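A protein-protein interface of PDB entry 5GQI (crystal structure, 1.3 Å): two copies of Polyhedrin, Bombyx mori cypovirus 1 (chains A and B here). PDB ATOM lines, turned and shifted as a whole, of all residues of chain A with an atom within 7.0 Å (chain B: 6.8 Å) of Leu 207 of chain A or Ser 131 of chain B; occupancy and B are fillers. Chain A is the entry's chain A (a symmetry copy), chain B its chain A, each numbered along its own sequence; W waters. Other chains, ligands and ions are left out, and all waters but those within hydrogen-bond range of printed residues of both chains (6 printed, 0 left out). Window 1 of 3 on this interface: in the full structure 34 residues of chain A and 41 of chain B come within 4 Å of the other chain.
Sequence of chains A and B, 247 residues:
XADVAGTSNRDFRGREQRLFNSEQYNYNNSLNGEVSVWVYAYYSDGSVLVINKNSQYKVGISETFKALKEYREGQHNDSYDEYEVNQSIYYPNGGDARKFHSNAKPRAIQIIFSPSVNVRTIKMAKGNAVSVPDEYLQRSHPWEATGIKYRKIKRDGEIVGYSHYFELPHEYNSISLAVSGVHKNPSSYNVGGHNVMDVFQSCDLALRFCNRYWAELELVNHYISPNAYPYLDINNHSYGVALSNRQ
Among the printed residues, merely in contact across the chains: Glu 34 of chain A with Pro 133 of chain B (3.2 Å), Glu 34 of chain A with Leu 137 of chain B (3.8 Å), Glu 34 of chain A with Pro 142 of chain B (3.8 Å), Asn 54 of chain A with Leu 137 of chain B (3.5 Å), Asp 204 of chain A with Ser 62 of chain B (3.3 Å), Asp 204 of chain A with Ala 178 of chain B (3.5 Å), Leu 205 of chain A with Ala 125 of chain B (3.8 Å), Leu 205 of chain A with Ala 178 of chain B (3.5 Å), Leu 207 of chain A with Ala 125 of chain B (3.7 Å), Leu 207 of chain A with Ser 131 of chain B (3.6 Å), Leu 207 of chain A with Pro 133 of chain B (3.97 Å), Leu 207 of chain A with Leu 177 of chain B (3.9 Å), Leu 207 of chain A with Ala 178 of chain B (3.8 Å), Arg 208 of chain A with Thr 64 of chain B (3.1 Å), Phe 209 of chain A with Ala 129 of chain B (3.8 Å), Phe 209 of chain A with Val 130 of chain B (3.7 Å), Phe 209 of chain A with Ser 131 of chain B (3.6 Å), Tyr 229 of chain A with Val 130 of chain B (3.95 Å), Tyr 229 of chain A with Val 132 of chain B (3.2 Å) and Tyr 229 of chain A with Leu 137 of chain B (3.5 Å).
Leu 207 of chain A touches five residues of chain B.
Printed residues of chain A within 4 Å of Ser 131 of chain B: Asn 54, Leu 207, Arg 208 and Phe 209.
Of the printed residues of chain A, Leu 137 of chain B touches Glu 34 (3.8 Å), Asn 54 (3.5 Å) and Tyr 229 (3.5 Å).
Of the printed residues of chain A, Val 132 of chain B touches Tyr 229 (3.2 Å).
Of the printed residues of chain B, Leu 205 of chain A touches Ala 125 and Ala 178.
Phe 65 of chain B touches none of the printed residues of chain A.
Gly 127 of chain B touches none of the printed residues of chain A.
The nearest printed residue of chain A that does not touch Ala 125 of chain B is Ala 206 of chain A (6.0 Å).
The side-chain amide oxygen of Asn 128 of chain B lies within hydrogen-bond range of the backbone NH of Val 132 of chain B (3.1 Å).
OD1 of Asn 128 of chain B is in hydrogen-bond range of N of Ser 131 of chain B, at 3.1 Å.
ND2 of Asn 54 of chain A is in hydrogen-bond range of OD1 of Asn 52 of chain A (2.9 Å).
O of Ala 178 of chain B sits at hydrogen-bond distance from N of Ala 125 of chain B (2.8 Å).
The backbone NH (N) of Asn 52 of chain A lies within hydrogen-bond range of the backbone carbonyl oxygen (O) of Phe 209 of chain A (2.8 Å).
N of Asn 54 of chain A lies within hydrogen-bond range of O of Leu 207 of chain A, at 2.9 Å.
Water W1 lies within hydrogen-bond range of the side-chain amide oxygen (OD1) of Asn 52 of chain A (2.6 Å), the backbone carbonyl oxygen (O) of Val 130 of chain B (2.7 Å) and the side-chain hydroxyl (OH) of Tyr 229 of chain A (2.8 Å).
Water W6 bridges O of Pro 142 of chain B (2.7 Å) and O of Leu 205 of chain A (2.7 Å).
Water W3 lies within hydrogen-bond range of OG1 of Thr 64 of chain B (2.7 Å) and SG of Cys 210 of chain A (3.7 Å).
Water W5 bridges OD1 of Asp 204 of chain A and N of Ser 62 of chain B.
Water W4 lies within hydrogen-bond range of OG of Ser 62 of chain B (2.8 Å), N of Arg 208 of chain A (2.9 Å) and O of Glu 63 of chain B (3.0 Å).
Water W2 lies within hydrogen-bond range of the backbone carbonyl oxygen of Leu 137 of chain B and the backbone NH of Glu 34 of chain A.
The backbone carbonyl oxygen (O) of Arg 208 of chain A is in hydrogen-bond range of the side-chain hydroxyl (OG) of Ser 131 of chain B, at 2.6 Å.
OG of Ser 62 of chain B is in hydrogen-bond range of O of Ala 206 of chain A (2.7 Å).
The backbone carbonyl oxygen of Ser 131 of chain B is in hydrogen-bond range of the side-chain amide nitrogen of Asn 54 of chain A (3.0 Å).
Of the 21 printed residues of chain B, 12 touch a printed residue of chain A.
Printed residues of chain B that touch a printed residue of chain A: Ser 62, Thr 64, Ala 125, Ala 129, Val 130, Ser 131, Val 132, Pro 133, Leu 137, Pro 142, Leu 177 and Ala 178.
Of the 16 printed residues of chain A, 9 touch a printed residue of chain B.
Hydrophobic or aromatic side chains of chain A that line the printed part of chain B: Leu 205, Leu 207, Phe 209 and Tyr 229.
Among the printed residues, 23 pairs touch across the chains.
Among the printed residues, no Asp or Glu carboxylate lies within 4 Å of a Lys or Arg side-chain nitrogen of the other chain.
No position is printed for both chains.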
ATOM      1  N   GLU A  34      12.409  24.438 -15.173  1.00  0.00           N
ATOM      2  CA  GLU A  34      13.793  24.282 -14.682  1.00  0.00           C
ATOM      3  C   GLU A  34      14.833  24.806 -15.626  1.00  0.00           C
ATOM      4  O   GLU A  34      14.656  24.807 -16.854  1.00  0.00           O
ATOM      5  CB  GLU A  34      14.092  22.775 -14.562  1.00  0.00           C
ATOM      6  CG  GLU A  34      13.301  22.022 -13.488  1.00  0.00           C
ATOM      7  CD  GLU A  34      13.901  22.211 -12.094  1.00  0.00           C
ATOM      8  OE1 GLU A  34      14.749  23.068 -11.802  1.00  0.00           O
ATOM      9  OE2 GLU A  34      13.302  21.610 -11.153  1.00  0.00           O
ATOM     10  N   ASN A  52      25.154  17.970  -9.963  1.00  0.00           N
ATOM     11  CA  ASN A  52      24.081  18.573 -10.752  1.00  0.00           C
ATOM     12  C   ASN A  52      23.329  19.526  -9.813  1.00  0.00           C
ATOM     13  O   ASN A  52      23.088  19.222  -8.640  1.00  0.00           O
ATOM     14  CB  ASN A  52      23.162  17.410 -11.144  1.00  0.00           C
ATOM     15  CG  ASN A  52      21.809  17.794 -11.746  1.00  0.00           C
ATOM     16  OD1 ASN A  52      20.842  17.096 -11.456  1.00  0.00           O
ATOM     17  ND2 ASN A  52      21.733  18.769 -12.608  1.00  0.00           N
ATOM     18  N   LYS A  53      22.856  20.642 -10.373  1.00  0.00           N
ATOM     19  CA  LYS A  53      21.896  21.554  -9.637  1.00  0.00           C
ATOM     20  C   LYS A  53      20.781  21.816 -10.612  1.00  0.00           C
ATOM     21  O   LYS A  53      20.994  22.106 -11.795  1.00  0.00           O
ATOM     22  CB  LYS A  53      22.670  22.879  -9.270  1.00  0.00           C
ATOM     23  CG  LYS A  53      21.913  23.720  -8.296  1.00  0.00           C
ATOM     24  CD  LYS A  53      22.304  23.334  -6.844  1.00  0.00           C
ATOM     25  CE  LYS A  53      23.629  23.949  -6.430  1.00  0.00           C
ATOM     26  NZ  LYS A  53      23.649  25.397  -6.063  1.00  0.00           N
ATOM     27  N   ASN A  54      19.557  21.737 -10.093  1.00  0.00           N
ATOM     28  CA  ASN A  54      18.344  22.020 -10.899  1.00  0.00           C
ATOM     29  C   ASN A  54      17.562  23.103 -10.184  1.00  0.00           C
ATOM     30  O   ASN A  54      17.185  22.919  -8.994  1.00  0.00           O
ATOM     31  CB  ASN A  54      17.465  20.702 -10.941  1.00  0.00           C
ATOM     32  CG  ASN A  54      18.249  19.560 -11.548  1.00  0.00           C
ATOM     33  OD1 ASN A  54      18.873  19.754 -12.616  1.00  0.00           O
ATOM     34  ND2 ASN A  54      18.347  18.419 -10.854  1.00  0.00           N
ATOM     35  N   SER A  55      17.285  24.220 -10.880  1.00  0.00           N
ATOM     36  CA  SER A  55      16.520  25.270 -10.162  1.00  0.00           C
ATOM     37  C   SER A  55      15.757  26.120 -11.170  1.00  0.00           C
ATOM     38  O   SER A  55      16.098  26.233 -12.377  1.00  0.00           O
ATOM     39  CB  SER A  55      17.483  26.190  -9.411  1.00  0.00           C
ATOM     40  OG  SER A  55      16.757  26.867  -8.352  1.00  0.00           O
ATOM     41  N   VAL A  59      20.780  29.040 -12.203  1.00  0.00           N
ATOM     42  CA  VAL A  59      21.331  27.896 -11.495  1.00  0.00           C
ATOM     43  C   VAL A  59      22.875  27.887 -11.602  1.00  0.00           C
ATOM     44  O   VAL A  59      23.440  28.438 -12.568  1.00  0.00           O
ATOM     45  CB  VAL A  59      20.762  26.561 -12.108  1.00  0.00           C
ATOM     46  CG1 VAL A  59      21.321  26.283 -13.511  1.00  0.00           C
ATOM     47  CG2 VAL A  59      20.979  25.421 -11.086  1.00  0.00           C
ATOM     48  N   SER A 202      14.130  30.629  -4.896  1.00  0.00           N
ATOM     49  CA  SER A 202      14.723  29.624  -5.785  1.00  0.00           C
ATOM     50  C   SER A 202      16.139  29.266  -5.344  1.00  0.00           C
ATOM     51  O   SER A 202      16.594  28.137  -5.597  1.00  0.00           O
ATOM     52  CB  SER A 202      14.673  30.002  -7.288  1.00  0.00           C
ATOM     53  OG  SER A 202      15.739  30.978  -7.618  1.00  0.00           O
ATOM     54  N   CYS A 203      16.882  30.194  -4.706  1.00  0.00           N
ATOM     55  CA  CYS A 203      18.248  29.890  -4.239  1.00  0.00           C
ATOM     56  C   CYS A 203      18.134  28.808  -3.135  1.00  0.00           C
ATOM     57  O   CYS A 203      19.043  27.980  -3.027  1.00  0.00           O
ATOM     58  CB  CYS A 203      18.842  31.153  -3.646  1.00  0.00           C
ATOM     59  SG  CYS A 203      19.148  32.402  -4.940  1.00  0.00           S
ATOM     60  N   ASP A 204      17.055  28.800  -2.338  1.00  0.00           N
ATOM     61  CA  ASP A 204      16.860  27.748  -1.340  1.00  0.00           C
ATOM     62  C   ASP A 204      16.268  26.473  -1.899  1.00  0.00           C
ATOM     63  O   ASP A 204      16.531  25.414  -1.332  1.00  0.00           O
ATOM     64  CB  ASP A 204      16.006  28.306  -0.213  1.00  0.00           C
ATOM     65  CG  ASP A 204      16.890  29.204   0.693  1.00  0.00           C
ATOM     66  OD1 ASP A 204      18.001  28.841   1.147  1.00  0.00           O
ATOM     67  OD2 ASP A 204      16.546  30.289   0.827  1.00  0.00           O
ATOM     68  N   LEU A 205      15.469  26.578  -2.970  1.00  0.00           N
ATOM     69  CA  LEU A 205      14.713  25.463  -3.531  1.00  0.00           C
ATOM     70  C   LEU A 205      15.509  24.608  -4.535  1.00  0.00           C
ATOM     71  O   LEU A 205      15.080  23.509  -4.829  1.00  0.00           O
ATOM     72  CB  LEU A 205      13.430  25.982  -4.156  1.00  0.00           C
ATOM     73  CG  LEU A 205      12.387  26.499  -3.135  1.00  0.00           C
ATOM     74  CD1 LEU A 205      11.336  27.375  -3.859  1.00  0.00           C
ATOM     75  CD2 LEU A 205      11.754  25.367  -2.294  1.00  0.00           C
ATOM     76  N   ALA A 206      16.623  25.185  -4.975  1.00  0.00           N
ATOM     77  CA  ALA A 206      17.468  24.475  -5.972  1.00  0.00           C
ATOM     78  C   ALA A 206      17.803  23.114  -5.396  1.00  0.00           C
ATOM     79  O   ALA A 206      18.265  23.022  -4.229  1.00  0.00           O
ATOM     80  CB  ALA A 206      18.752  25.271  -6.236  1.00  0.00           C
ATOM     81  N   LEU A 207      17.641  22.041  -6.164  1.00  0.00           N
ATOM     82  CA  LEU A 207      18.012  20.671  -5.709  1.00  0.00           C
ATOM     83  C   LEU A 207      19.409  20.319  -6.233  1.00  0.00           C
ATOM     84  O   LEU A 207      19.746  20.646  -7.412  1.00  0.00           O
ATOM     85  CB  LEU A 207      17.000  19.636  -6.233  1.00  0.00           C
ATOM     86  CG  LEU A 207      15.592  19.754  -5.548  1.00  0.00           C
ATOM     87  CD1 LEU A 207      14.691  18.733  -6.173  1.00  0.00           C
ATOM     88  CD2 LEU A 207      15.658  19.508  -4.036  1.00  0.00           C
ATOM     89  N   ARG A 208      20.216  19.708  -5.373  1.00  0.00           N
ATOM     90  CA  ARG A 208      21.579  19.297  -5.715  1.00  0.00           C
ATOM     91  C   ARG A 208      21.649  17.797  -5.737  1.00  0.00           C
ATOM     92  O   ARG A 208      20.991  17.096  -4.978  1.00  0.00           O
ATOM     93  CB  ARG A 208      22.528  19.903  -4.660  1.00  0.00           C
ATOM     94  CG  ARG A 208      24.022  19.580  -4.979  1.00  0.00           C
ATOM     95  CD  ARG A 208      24.906  20.569  -4.159  1.00  0.00           C
ATOM     96  NE  ARG A 208      26.369  20.454  -4.384  1.00  0.00           N
ATOM     97  CZ  ARG A 208      27.061  19.481  -3.852  1.00  0.00           C
ATOM     98  NH1 ARG A 208      26.390  18.592  -3.122  1.00  0.00           N
ATOM     99  NH2 ARG A 208      28.375  19.364  -4.056  1.00  0.00           N
ATOM    100  N   PHE A 209      22.564  17.280  -6.610  1.00  0.00           N
ATOM    101  CA  PHE A 209      22.871  15.835  -6.567  1.00  0.00           C
ATOM    102  C   PHE A 209      24.353  15.709  -6.788  1.00  0.00           C
ATOM    103  O   PHE A 209      24.955  16.426  -7.651  1.00  0.00           O
ATOM    104  CB  PHE A 209      22.133  15.176  -7.738  1.00  0.00           C
ATOM    105  CG  PHE A 209      22.531  13.717  -7.945  1.00  0.00           C
ATOM    106  CD1 PHE A 209      21.908  12.675  -7.190  1.00  0.00           C
ATOM    107  CD2 PHE A 209      23.507  13.385  -8.884  1.00  0.00           C
ATOM    108  CE1 PHE A 209      22.300  11.314  -7.402  1.00  0.00           C
ATOM    109  CE2 PHE A 209      23.864  12.058  -9.086  1.00  0.00           C
ATOM    110  CZ  PHE A 209      23.277  11.046  -8.332  1.00  0.00           C
ATOM    111  N   CYS A 210      25.001  14.794  -6.077  1.00  0.00           N
ATOM    112  CA  CYS A 210      26.397  14.452  -6.409  1.00  0.00           C
ATOM    113  C   CYS A 210      26.667  13.002  -6.134  1.00  0.00           C
ATOM    114  O   CYS A 210      26.211  12.409  -5.161  1.00  0.00           O
ATOM    115  CB  CYS A 210      27.416  15.352  -5.738  1.00  0.00           C
ATOM    116  SG  CYS A 210      27.389  15.301  -3.997  1.00  0.00           S
ATOM    117  N   TYR A 229      18.596  13.040 -19.604  1.00  0.00           N
ATOM    118  CA  TYR A 229      19.562  14.156 -19.591  1.00  0.00           C
ATOM    119  C   TYR A 229      20.380  14.170 -20.863  1.00  0.00           C
ATOM    120  O   TYR A 229      20.579  13.133 -21.514  1.00  0.00           O
ATOM    121  CB  TYR A 229      20.532  13.973 -18.436  1.00  0.00           C
ATOM    122  CG  TYR A 229      19.958  14.052 -17.066  1.00  0.00           C
ATOM    123  CD1 TYR A 229      18.714  14.647 -16.794  1.00  0.00           C
ATOM    124  CD2 TYR A 229      20.714  13.576 -15.978  1.00  0.00           C
ATOM    125  CE1 TYR A 229      18.233  14.759 -15.481  1.00  0.00           C
ATOM    126  CE2 TYR A 229      20.248  13.709 -14.640  1.00  0.00           C
ATOM    127  CZ  TYR A 229      19.001  14.300 -14.452  1.00  0.00           C
ATOM    128  OH  TYR A 229      18.492  14.455 -13.161  1.00  0.00           O
ATOM    129  N   SER B  62      18.093  22.968   1.716  1.00  0.00           N
ATOM    130  CA  SER B  62      18.095  22.071   0.533  1.00  0.00           C
ATOM    131  C   SER B  62      19.076  20.963   0.785  1.00  0.00           C
ATOM    132  O   SER B  62      20.225  21.284   1.110  1.00  0.00           O
ATOM    133  CB  SER B  62      18.489  22.856  -0.742  1.00  0.00           C
ATOM    134  OG  SER B  62      18.473  21.887  -1.811  1.00  0.00           O
ATOM    135  N   GLU B  63      18.636  19.705   0.692  1.00  0.00           N
ATOM    136  CA  GLU B  63      19.538  18.550   0.969  1.00  0.00           C
ATOM    137  C   GLU B  63      19.391  17.495  -0.096  1.00  0.00           C
ATOM    138  O   GLU B  63      18.295  17.268  -0.649  1.00  0.00           O
ATOM    139  CB  GLU B  63      19.298  17.948   2.344  1.00  0.00           C
ATOM    140  CG  GLU B  63      19.454  19.043   3.493  1.00  0.00           C
ATOM    141  CD  GLU B  63      20.885  19.478   3.710  1.00  0.00           C
ATOM    142  OE1 GLU B  63      21.831  18.794   3.282  1.00  0.00           O
ATOM    143  OE2 GLU B  63      21.102  20.545   4.347  1.00  0.00           O
ATOM    144  N   THR B  64      20.493  16.804  -0.356  1.00  0.00           N
ATOM    145  CA  THR B  64      20.464  15.664  -1.263  1.00  0.00           C
ATOM    146  C   THR B  64      19.845  14.424  -0.580  1.00  0.00           C
ATOM    147  O   THR B  64      19.759  14.388   0.707  1.00  0.00           O
ATOM    148  CB  THR B  64      21.897  15.317  -1.702  1.00  0.00           C
ATOM    149  OG1 THR B  64      22.633  14.803  -0.573  1.00  0.00           O
ATOM    150  CG2 THR B  64      22.615  16.552  -2.350  1.00  0.00           C
ATOM    151  N   PHE B  65      19.443  13.383  -1.379  1.00  0.00           N
ATOM    152  CA  PHE B  65      19.067  12.136  -0.766  1.00  0.00           C
ATOM    153  C   PHE B  65      20.139  11.593   0.191  1.00  0.00           C
ATOM    154  O   PHE B  65      19.842  11.184   1.327  1.00  0.00           O
ATOM    155  CB  PHE B  65      18.883  11.115  -1.921  1.00  0.00           C
ATOM    156  CG  PHE B  65      18.743   9.692  -1.433  1.00  0.00           C
ATOM    157  CD1 PHE B  65      17.571   9.244  -0.832  1.00  0.00           C
ATOM    158  CD2 PHE B  65      19.849   8.843  -1.448  1.00  0.00           C
ATOM    159  CE1 PHE B  65      17.484   7.950  -0.297  1.00  0.00           C
ATOM    160  CE2 PHE B  65      19.726   7.504  -0.885  1.00  0.00           C
ATOM    161  CZ  PHE B  65      18.545   7.085  -0.340  1.00  0.00           C
ATOM    162  N   ALA B 125      10.301  21.612  -2.704  1.00  0.00           N
ATOM    163  CA  ALA B 125      10.738  20.761  -3.784  1.00  0.00           C
ATOM    164  C   ALA B 125      11.062  19.391  -3.221  1.00  0.00           C
ATOM    165  O   ALA B 125      12.196  19.192  -2.681  1.00  0.00           O
ATOM    166  CB  ALA B 125      11.961  21.384  -4.497  1.00  0.00           C
ATOM    167  N   LYS B 126      10.133  18.457  -3.319  1.00  0.00           N
ATOM    168  CA  LYS B 126      10.362  17.106  -2.831  1.00  0.00           C
ATOM    169  C   LYS B 126      10.696  16.304  -4.054  1.00  0.00           C
ATOM    170  O   LYS B 126       9.813  15.975  -4.895  1.00  0.00           O
ATOM    171  CB  LYS B 126       9.098  16.615  -2.057  1.00  0.00           C
ATOM    172  CG  LYS B 126       9.225  15.169  -1.581  1.00  0.00           C
ATOM    173  CD  LYS B 126       8.009  14.698  -0.810  1.00  0.00           C
ATOM    174  CE  LYS B 126       6.666  14.595  -1.522  1.00  0.00           C
ATOM    175  NZ  LYS B 126       6.527  13.422  -2.404  1.00  0.00           N
ATOM    176  N   GLY B 127      11.982  16.043  -4.237  1.00  0.00           N
ATOM    177  CA  GLY B 127      12.504  15.381  -5.436  1.00  0.00           C
ATOM    178  C   GLY B 127      12.617  13.908  -5.242  1.00  0.00           C
ATOM    179  O   GLY B 127      12.512  13.387  -4.121  1.00  0.00           O
ATOM    180  N   ASN B 128      12.814  13.244  -6.347  1.00  0.00           N
ATOM    181  CA  ASN B 128      13.217  11.832  -6.268  1.00  0.00           C
ATOM    182  C   ASN B 128      14.714  11.736  -5.860  1.00  0.00           C
ATOM    183  O   ASN B 128      15.386  12.724  -5.522  1.00  0.00           O
ATOM    184  CB  ASN B 128      12.948  11.061  -7.602  1.00  0.00           C
ATOM    185  CG  ASN B 128      13.796  11.576  -8.744  1.00  0.00           C
ATOM    186  OD1 ASN B 128      14.803  12.293  -8.570  1.00  0.00           O
ATOM    187  ND2 ASN B 128      13.455  11.159  -9.977  1.00  0.00           N
ATOM    188  N   ALA B 129      15.228  10.522  -5.839  1.00  0.00           N
ATOM    189  CA  ALA B 129      16.571  10.348  -5.284  1.00  0.00           C
ATOM    190  C   ALA B 129      17.679  10.964  -6.097  1.00  0.00           C
ATOM    191  O   ALA B 129      18.814  11.109  -5.579  1.00  0.00           O
ATOM    192  CB  ALA B 129      16.876   8.868  -4.966  1.00  0.00           C
ATOM    193  N   VAL B 130      17.401  11.290  -7.361  1.00  0.00           N
ATOM    194  CA  VAL B 130      18.437  11.979  -8.218  1.00  0.00           C
ATOM    195  C   VAL B 130      18.121  13.468  -8.321  1.00  0.00           C
ATOM    196  O   VAL B 130      18.623  14.120  -9.226  1.00  0.00           O
ATOM    197  CB  VAL B 130      18.661  11.276  -9.583  1.00  0.00           C
ATOM    198  CG1 VAL B 130      19.203   9.871  -9.317  1.00  0.00           C
ATOM    199  CG2 VAL B 130      17.316  11.173 -10.395  1.00  0.00           C
ATOM    200  N   SER B 131      17.224  13.964  -7.447  1.00  0.00           N
ATOM    201  CA  SER B 131      17.079  15.458  -7.287  1.00  0.00           C
ATOM    202  C   SER B 131      16.307  16.066  -8.416  1.00  0.00           C
ATOM    203  O   SER B 131      16.551  17.193  -8.809  1.00  0.00           O
ATOM    204  CB  SER B 131      18.430  16.172  -7.070  1.00  0.00           C
ATOM    205  OG  SER B 131      19.038  15.557  -5.869  1.00  0.00           O
ATOM    206  N   VAL B 132      15.287  15.322  -8.885  1.00  0.00           N
ATOM    207  CA  VAL B 132      14.353  15.812  -9.901  1.00  0.00           C
ATOM    208  C   VAL B 132      12.976  15.976  -9.206  1.00  0.00           C
ATOM    209  O   VAL B 132      12.458  15.002  -8.648  1.00  0.00           O
ATOM    210  CB  VAL B 132      14.274  14.829 -11.081  1.00  0.00           C
ATOM    211  CG1 VAL B 132      13.198  15.262 -12.113  1.00  0.00           C
ATOM    212  CG2 VAL B 132      15.677  14.812 -11.741  1.00  0.00           C
ATOM    213  N   PRO B 133      12.336  17.180  -9.341  1.00  0.00           N
ATOM    214  CA  PRO B 133      11.076  17.368  -8.574  1.00  0.00           C
ATOM    215  C   PRO B 133       9.968  16.510  -9.027  1.00  0.00           C
ATOM    216  O   PRO B 133       9.182  16.080  -8.162  1.00  0.00           O
ATOM    217  CB  PRO B 133      10.765  18.854  -8.844  1.00  0.00           C
ATOM    218  CG  PRO B 133      12.082  19.534  -9.056  1.00  0.00           C
ATOM    219  CD  PRO B 133      12.893  18.456  -9.858  1.00  0.00           C
ATOM    220  N   ASP B 134       9.807  16.171 -10.307  1.00  0.00           N
ATOM    221  CA  ASP B 134       8.627  15.494 -10.729  1.00  0.00           C
ATOM    222  C   ASP B 134       8.907  14.622 -11.967  1.00  0.00           C
ATOM    223  O   ASP B 134       8.568  15.013 -13.136  1.00  0.00           O
ATOM    224  CB  ASP B 134       7.535  16.566 -11.008  1.00  0.00           C
ATOM    225  CG  ASP B 134       6.175  15.937 -11.228  1.00  0.00           C
ATOM    226  OD1 ASP B 134       6.053  14.673 -11.107  1.00  0.00           O
ATOM    227  OD2 ASP B 134       5.220  16.694 -11.615  1.00  0.00           O
ATOM    228  N   LEU B 137      13.073  16.393 -15.582  1.00  0.00           N
ATOM    229  CA  LEU B 137      13.212  17.825 -15.419  1.00  0.00           C
ATOM    230  C   LEU B 137      12.347  18.631 -16.370  1.00  0.00           C
ATOM    231  O   LEU B 137      11.796  19.676 -16.045  1.00  0.00           O
ATOM    232  CB  LEU B 137      14.662  18.238 -15.746  1.00  0.00           C
ATOM    233  CG  LEU B 137      15.682  17.773 -14.660  1.00  0.00           C
ATOM    234  CD1 LEU B 137      17.098  18.022 -15.188  1.00  0.00           C
ATOM    235  CD2 LEU B 137      15.482  18.540 -13.343  1.00  0.00           C
ATOM    236  N   PRO B 142       9.426  23.559 -10.411  1.00  0.00           N
ATOM    237  CA  PRO B 142      10.500  23.394  -9.402  1.00  0.00           C
ATOM    238  C   PRO B 142      10.061  23.371  -7.936  1.00  0.00           C
ATOM    239  O   PRO B 142      10.890  23.207  -7.057  1.00  0.00           O
ATOM    240  CB  PRO B 142      11.462  24.559  -9.688  1.00  0.00           C
ATOM    241  CG  PRO B 142      11.215  24.801 -11.172  1.00  0.00           C
ATOM    242  CD  PRO B 142       9.732  24.736 -11.287  1.00  0.00           C
ATOM    243  N   ILE B 175      13.784  10.184  -1.246  1.00  0.00           N
ATOM    244  CA  ILE B 175      13.653  11.622  -1.620  1.00  0.00           C
ATOM    245  C   ILE B 175      14.891  12.437  -1.447  1.00  0.00           C
ATOM    246  O   ILE B 175      15.805  12.144  -0.646  1.00  0.00           O
ATOM    247  CB  ILE B 175      12.487  12.302  -0.820  1.00  0.00           C
ATOM    248  CG1 ILE B 175      12.827  12.430   0.671  1.00  0.00           C
ATOM    249  CG2 ILE B 175      11.167  11.559  -1.034  1.00  0.00           C
ATOM    250  CD1 ILE B 175      11.901  13.467   1.395  1.00  0.00           C
ATOM    251  N   SER B 176      14.900  13.516  -2.254  1.00  0.00           N
ATOM    252  CA  SER B 176      15.723  14.702  -1.953  1.00  0.00           C
ATOM    253  C   SER B 176      14.734  15.784  -1.558  1.00  0.00           C
ATOM    254  O   SER B 176      13.552  15.678  -1.819  1.00  0.00           O
ATOM    255  CB  SER B 176      16.436  15.094  -3.262  1.00  0.00           C
ATOM    256  OG  SER B 176      15.529  15.230  -4.364  1.00  0.00           O
ATOM    257  N   LEU B 177      15.245  16.846  -0.887  1.00  0.00           N
ATOM    258  CA  LEU B 177      14.250  17.773  -0.306  1.00  0.00           C
ATOM    259  C   LEU B 177      14.838  19.178  -0.221  1.00  0.00           C
ATOM    260  O   LEU B 177      15.907  19.406   0.368  1.00  0.00           O
ATOM    261  CB  LEU B 177      13.882  17.274   1.099  1.00  0.00           C
ATOM    262  CG  LEU B 177      12.817  18.129   1.815  1.00  0.00           C
ATOM    263  CD1 LEU B 177      11.471  18.109   1.094  1.00  0.00           C
ATOM    264  CD2 LEU B 177      12.626  17.611   3.263  1.00  0.00           C
ATOM    265  N   ALA B 178      14.013  20.151  -0.673  1.00  0.00           N
ATOM    266  CA  ALA B 178      14.234  21.548  -0.335  1.00  0.00           C
ATOM    267  C   ALA B 178      12.944  22.196   0.055  1.00  0.00           C
ATOM    268  O   ALA B 178      11.878  21.844  -0.427  1.00  0.00           O
ATOM    269  CB  ALA B 178      14.877  22.347  -1.508  1.00  0.00           C
ATOM    270  N   VAL B 179      13.071  23.165   0.956  1.00  0.00           N
ATOM    271  CA  VAL B 179      11.880  23.885   1.431  1.00  0.00           C
ATOM    272  C   VAL B 179      12.261  25.315   1.703  1.00  0.00           C
ATOM    273  O   VAL B 179      13.438  25.642   1.975  1.00  0.00           O
ATOM    274  CB  VAL B 179      11.256  23.240   2.702  1.00  0.00           C
ATOM    275  CG1 VAL B 179      12.271  23.216   3.866  1.00  0.00           C
ATOM    276  CG2 VAL B 179       9.813  23.726   2.946  1.00  0.00           C
HETATM  277  O   HOH W   1      20.442  14.511 -11.190  1.00  0.00           O
HETATM  278  O   HOH W   2      10.771  22.270 -16.155  1.00  0.00           O
HETATM  279  O   HOH W   3      25.309  14.706  -1.006  1.00  0.00           O
HETATM  280  O   HOH W   4      19.273  19.356  -2.635  1.00  0.00           O
HETATM  281  O   HOH W   5      18.675  26.194   1.081  1.00  0.00           O
HETATM  282  O   HOH W   6      13.566  23.601  -7.122  1.00  0.00           O
